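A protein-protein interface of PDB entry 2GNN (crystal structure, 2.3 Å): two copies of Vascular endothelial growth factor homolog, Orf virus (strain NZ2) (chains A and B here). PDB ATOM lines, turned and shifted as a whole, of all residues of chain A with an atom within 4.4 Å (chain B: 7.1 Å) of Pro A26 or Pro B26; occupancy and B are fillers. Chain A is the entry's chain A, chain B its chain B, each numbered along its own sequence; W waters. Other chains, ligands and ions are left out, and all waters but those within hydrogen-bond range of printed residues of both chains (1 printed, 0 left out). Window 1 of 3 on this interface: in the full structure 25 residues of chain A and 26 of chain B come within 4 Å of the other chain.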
ATOM      1  N   ARG A  25       9.211 -23.571   4.050  1.00  0.00           N
ATOM      2  CA  ARG A  25      10.161 -24.414   4.765  1.00  0.00           C
ATOM      3  C   ARG A  25       9.441 -25.242   5.819  1.00  0.00           C
ATOM      4  O   ARG A  25       8.471 -24.769   6.411  1.00  0.00           O
ATOM      5  CB  ARG A  25      11.228 -23.523   5.400  1.00  0.00           C
ATOM      6  CG  ARG A  25      12.161 -22.905   4.365  1.00  0.00           C
ATOM      7  CD  ARG A  25      12.774 -21.687   4.926  1.00  0.00           C
ATOM      8  NE  ARG A  25      13.751 -21.078   4.034  1.00  0.00           N
ATOM      9  CZ  ARG A  25      14.970 -21.551   3.797  1.00  0.00           C
ATOM     10  NH1 ARG A  25      15.392 -22.678   4.361  1.00  0.00           N
ATOM     11  NH2 ARG A  25      15.764 -20.890   2.970  1.00  0.00           N
ATOM     12  N   PRO A  26       9.900 -26.488   6.055  1.00  0.00           N
ATOM     13  CA  PRO A  26       9.232 -27.297   7.064  1.00  0.00           C
ATOM     14  C   PRO A  26       9.594 -26.806   8.464  1.00  0.00           C
ATOM     15  O   PRO A  26      10.769 -26.570   8.742  1.00  0.00           O
ATOM     16  CB  PRO A  26       9.796 -28.698   6.811  1.00  0.00           C
ATOM     17  CG  PRO A  26      11.146 -28.461   6.234  1.00  0.00           C
ATOM     18  CD  PRO A  26      11.046 -27.194   5.443  1.00  0.00           C
ATOM     19  N   ILE A  27       8.597 -26.611   9.324  1.00  0.00           N
ATOM     20  CA  ILE A  27       8.864 -26.227  10.707  1.00  0.00           C
ATOM     21  C   ILE A  27       8.007 -27.035  11.687  1.00  0.00           C
ATOM     22  O   ILE A  27       6.871 -27.384  11.386  1.00  0.00           O
ATOM     23  CB  ILE A  27       8.776 -24.672  10.951  1.00  0.00           C
ATOM     24  CG1 ILE A  27       7.344 -24.165  11.019  1.00  0.00           C
ATOM     25  CG2 ILE A  27       9.571 -23.874   9.924  1.00  0.00           C
ATOM     26  CD1 ILE A  27       7.016 -23.639  12.397  1.00  0.00           C
ATOM     27  N   THR A  49       4.933 -31.263  11.524  1.00  0.00           N
ATOM     28  CA  THR A  49       5.656 -30.419  10.567  1.00  0.00           C
ATOM     29  C   THR A  49       4.668 -29.748   9.599  1.00  0.00           C
ATOM     30  O   THR A  49       3.866 -30.429   8.950  1.00  0.00           O
ATOM     31  CB  THR A  49       6.741 -31.214   9.799  1.00  0.00           C
ATOM     32  OG1 THR A  49       7.815 -31.519  10.687  1.00  0.00           O
ATOM     33  CG2 THR A  49       7.303 -30.414   8.665  1.00  0.00           C
ATOM     34  N   LEU A  50       4.720 -28.415   9.545  1.00  0.00           N
ATOM     35  CA  LEU A  50       3.945 -27.599   8.615  1.00  0.00           C
ATOM     36  C   LEU A  50       4.892 -26.816   7.732  1.00  0.00           C
ATOM     37  O   LEU A  50       5.912 -26.315   8.209  1.00  0.00           O
ATOM     38  CB  LEU A  50       3.048 -26.596   9.354  1.00  0.00           C
ATOM     39  CG  LEU A  50       1.957 -27.122  10.279  1.00  0.00           C
ATOM     40  CD1 LEU A  50       1.232 -25.963  10.915  1.00  0.00           C
ATOM     41  CD2 LEU A  50       0.984 -28.031   9.535  1.00  0.00           C
ATOM     42  N   MET A  51       4.554 -26.704   6.452  1.00  0.00           N
ATOM     43  CA  MET A  51       5.289 -25.827   5.553  1.00  0.00           C
ATOM     44  C   MET A  51       4.886 -24.395   5.838  1.00  0.00           C
ATOM     45  O   MET A  51       3.707 -24.073   5.866  1.00  0.00           O
ATOM     46  CB  MET A  51       5.024 -26.178   4.101  1.00  0.00           C
ATOM     47  CG  MET A  51       5.314 -27.643   3.768  1.00  0.00           C
ATOM     48  SD  MET A  51       7.058 -28.059   3.922  1.00  0.00           S
ATOM     49  CE  MET A  51       7.843 -26.791   2.935  1.00  0.00           C
ATOM     50  N   LYS B  23      14.793 -35.748  14.965  1.00  0.00           N
ATOM     51  CA  LYS B  23      15.750 -36.078  13.919  1.00  0.00           C
ATOM     52  C   LYS B  23      16.323 -34.757  13.452  1.00  0.00           C
ATOM     53  O   LYS B  23      15.803 -33.704  13.834  1.00  0.00           O
ATOM     54  CB  LYS B  23      15.069 -36.816  12.759  1.00  0.00           C
ATOM     55  CG  LYS B  23      14.074 -35.959  11.970  1.00  0.00           C
ATOM     56  CD  LYS B  23      13.666 -36.625  10.672  1.00  0.00           C
ATOM     57  CE  LYS B  23      12.658 -35.763   9.911  1.00  0.00           C
ATOM     58  NZ  LYS B  23      12.351 -36.302   8.548  1.00  0.00           N
ATOM     59  N   PRO B  24      17.422 -34.792  12.671  1.00  0.00           N
ATOM     60  CA  PRO B  24      17.932 -33.527  12.125  1.00  0.00           C
ATOM     61  C   PRO B  24      16.947 -32.922  11.110  1.00  0.00           C
ATOM     62  O   PRO B  24      16.411 -33.631  10.266  1.00  0.00           O
ATOM     63  CB  PRO B  24      19.238 -33.935  11.433  1.00  0.00           C
ATOM     64  CG  PRO B  24      19.584 -35.283  11.997  1.00  0.00           C
ATOM     65  CD  PRO B  24      18.276 -35.936  12.292  1.00  0.00           C
ATOM     66  N   ARG B  25      16.715 -31.622  11.215  1.00  0.00           N
ATOM     67  CA  ARG B  25      15.789 -30.913  10.365  1.00  0.00           C
ATOM     68  C   ARG B  25      16.433 -29.594   9.980  1.00  0.00           C
ATOM     69  O   ARG B  25      17.162 -29.028  10.798  1.00  0.00           O
ATOM     70  CB  ARG B  25      14.507 -30.631  11.129  1.00  0.00           C
ATOM     71  CG  ARG B  25      13.726 -31.867  11.432  1.00  0.00           C
ATOM     72  CD  ARG B  25      12.741 -31.602  12.514  1.00  0.00           C
ATOM     73  NE  ARG B  25      12.040 -32.833  12.815  1.00  0.00           N
ATOM     74  CZ  ARG B  25      10.891 -33.191  12.263  1.00  0.00           C
ATOM     75  NH1 ARG B  25      10.290 -32.392  11.391  1.00  0.00           N
ATOM     76  NH2 ARG B  25      10.336 -34.343  12.593  1.00  0.00           N
ATOM     77  N   PRO B  26      16.159 -29.099   8.746  1.00  0.00           N
ATOM     78  CA  PRO B  26      16.663 -27.794   8.338  1.00  0.00           C
ATOM     79  C   PRO B  26      16.019 -26.691   9.167  1.00  0.00           C
ATOM     80  O   PRO B  26      14.833 -26.758   9.502  1.00  0.00           O
ATOM     81  CB  PRO B  26      16.246 -27.691   6.868  1.00  0.00           C
ATOM     82  CG  PRO B  26      15.076 -28.623   6.724  1.00  0.00           C
ATOM     83  CD  PRO B  26      15.365 -29.746   7.678  1.00  0.00           C
ATOM     84  N   ILE B  27      16.817 -25.699   9.521  1.00  0.00           N
ATOM     85  CA  ILE B  27      16.340 -24.561  10.277  1.00  0.00           C
ATOM     86  C   ILE B  27      17.131 -23.361   9.764  1.00  0.00           C
ATOM     87  O   ILE B  27      18.318 -23.482   9.437  1.00  0.00           O
ATOM     88  CB  ILE B  27      16.472 -24.791  11.833  1.00  0.00           C
ATOM     89  CG1 ILE B  27      15.726 -23.711  12.618  1.00  0.00           C
ATOM     90  CG2 ILE B  27      17.929 -24.843  12.287  1.00  0.00           C
ATOM     91  CD1 ILE B  27      15.131 -24.203  13.937  1.00  0.00           C
ATOM     92  N   VAL B  28      16.462 -22.220   9.632  1.00  0.00           N
ATOM     93  CA  VAL B  28      17.113 -21.006   9.157  1.00  0.00           C
ATOM     94  C   VAL B  28      17.684 -20.310  10.369  1.00  0.00           C
ATOM     95  O   VAL B  28      16.967 -20.059  11.336  1.00  0.00           O
ATOM     96  CB  VAL B  28      16.117 -20.068   8.402  1.00  0.00           C
ATOM     97  CG1 VAL B  28      16.799 -18.786   7.967  1.00  0.00           C
ATOM     98  CG2 VAL B  28      15.533 -20.781   7.201  1.00  0.00           C
ATOM     99  N   THR B  49      20.627 -22.047   6.100  1.00  0.00           N
ATOM    100  CA  THR B  49      19.919 -23.242   6.525  1.00  0.00           C
ATOM    101  C   THR B  49      20.914 -24.296   7.052  1.00  0.00           C
ATOM    102  O   THR B  49      21.819 -24.742   6.324  1.00  0.00           O
ATOM    103  CB  THR B  49      19.088 -23.822   5.370  1.00  0.00           C
ATOM    104  OG1 THR B  49      18.274 -22.792   4.828  1.00  0.00           O
ATOM    105  CG2 THR B  49      18.188 -24.930   5.847  1.00  0.00           C
ATOM    106  N   LEU B  50      20.725 -24.687   8.312  1.00  0.00           N
ATOM    107  CA  LEU B  50      21.559 -25.701   8.952  1.00  0.00           C
ATOM    108  C   LEU B  50      20.717 -26.876   9.407  1.00  0.00           C
ATOM    109  O   LEU B  50      19.571 -26.696   9.843  1.00  0.00           O
ATOM    110  CB  LEU B  50      22.273 -25.101  10.163  1.00  0.00           C
ATOM    111  CG  LEU B  50      23.246 -23.953   9.916  1.00  0.00           C
ATOM    112  CD1 LEU B  50      23.801 -23.457  11.226  1.00  0.00           C
ATOM    113  CD2 LEU B  50      24.359 -24.436   9.019  1.00  0.00           C
ATOM    114  N   MET B  51      21.276 -28.081   9.296  1.00  0.00           N
ATOM    115  CA  MET B  51      20.627 -29.266   9.841  1.00  0.00           C
ATOM    116  C   MET B  51      20.817 -29.267  11.352  1.00  0.00           C
ATOM    117  O   MET B  51      21.939 -29.246  11.848  1.00  0.00           O
ATOM    118  CB  MET B  51      21.190 -30.534   9.218  1.00  0.00           C
ATOM    119  CG  MET B  51      20.930 -30.656   7.732  1.00  0.00           C
ATOM    120  SD  MET B  51      19.179 -30.521   7.317  1.00  0.00           S
ATOM    121  CE  MET B  51      18.551 -32.132   7.795  1.00  0.00           C
ATOM    122  N   ARG B  52      19.713 -29.242  12.082  1.00  0.00           N
ATOM    123  CA  ARG B  52      19.759 -29.199  13.537  1.00  0.00           C
ATOM    124  C   ARG B  52      18.695 -30.106  14.090  1.00  0.00           C
ATOM    125  O   ARG B  52      17.644 -30.281  13.472  1.00  0.00           O
ATOM    126  CB  ARG B  52      19.479 -27.792  14.025  1.00  0.00           C
ATOM    127  CG  ARG B  52      20.653 -26.882  13.948  1.00  0.00           C
ATOM    128  CD  ARG B  52      21.317 -26.740  15.300  1.00  0.00           C
ATOM    129  NE  ARG B  52      22.441 -25.818  15.243  1.00  0.00           N
ATOM    130  CZ  ARG B  52      23.451 -25.947  14.391  1.00  0.00           C
ATOM    131  NH1 ARG B  52      23.437 -26.949  13.517  1.00  0.00           N
ATOM    132  NH2 ARG B  52      24.452 -25.068  14.389  1.00  0.00           N
ATOM    133  N   GLU B  94      26.556 -28.908  11.981  1.00  0.00           N
ATOM    134  CA  GLU B  94      25.294 -29.559  11.590  1.00  0.00           C
ATOM    135  C   GLU B  94      25.094 -30.791  12.457  1.00  0.00           C
ATOM    136  O   GLU B  94      26.062 -31.451  12.816  1.00  0.00           O
ATOM    137  CB  GLU B  94      25.338 -30.044  10.139  1.00  0.00           C
ATOM    138  CG  GLU B  94      25.855 -29.055   9.126  1.00  0.00           C
ATOM    139  CD  GLU B  94      24.760 -28.316   8.390  1.00  0.00           C
ATOM    140  OE1 GLU B  94      23.610 -28.789   8.341  1.00  0.00           O
ATOM    141  OE2 GLU B  94      25.061 -27.252   7.835  1.00  0.00           O
HETATM  142  O   HOH W   1      13.089 -24.955   8.052  1.00  0.00           O
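OG1 of Thr A49 sits at hydrogen-bond distance from NH1 of Arg B25, at 2.7 Å.
NH1 of Arg A25 sits at hydrogen-bond distance from OG1 of Thr B49.
The backbone carbonyl oxygen (O) of Arg B52 lies within hydrogen-bond range of the backbone NH (N) of Arg B25 (2.8 Å).
NH1 of Arg A25 touches CG2 of Val B28, 3.4 Å away.
Pro B26 touches Pro A26.
Of chain B, only Pro B26 (3.96 Å) comes within 4 Å of Pro A26.
Of chain A, only Pro A26 comes within 4 Å of Pro B26.
Printed residues of chain A within 4 Å of Arg B25: Thr A49 (2.7 Å).
Printed residues of chain B within 4 Å of Arg A25: Val B28 (3.4 Å) and Thr B49 (2.9 Å).
Printed residues of chain B within 4 Å of Thr A49: Arg B25.
Printed residues of chain A within 4 Å of Thr B49: Arg A25 (2.9 Å).
The nearest printed residue of chain A that does not touch Pro B26 is Arg A25 (5.7 Å).
The nearest printed residue of chain A that does not touch Val B28 is Ile A27 (7.1 Å).
Of the 11 printed residues of chain B, 4 touch a printed residue of chain A.
Of the 6 printed residues of chain A, 3 touch a printed residue of chain B.
Printed residues of chain A that touch a printed residue of chain B: Arg A25, Pro A26 and Thr A49.
Hydrophobic or aromatic side chains of chain A that line the printed part of chain B: Pro A26.
Arg A25 touches Thr B49, and with the chains exchanged Thr A49 touches Arg B25.
Pro B26 touches its own counterpart, Pro A26.
Of the 4 pairs that touch across the chains among the printed residues, 3 have their exchanged pair printed and touching as well.
Water W1 lies within hydrogen-bond range of O of Pro B26 (2.9 Å) and O of Pro A26 (2.9 Å).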
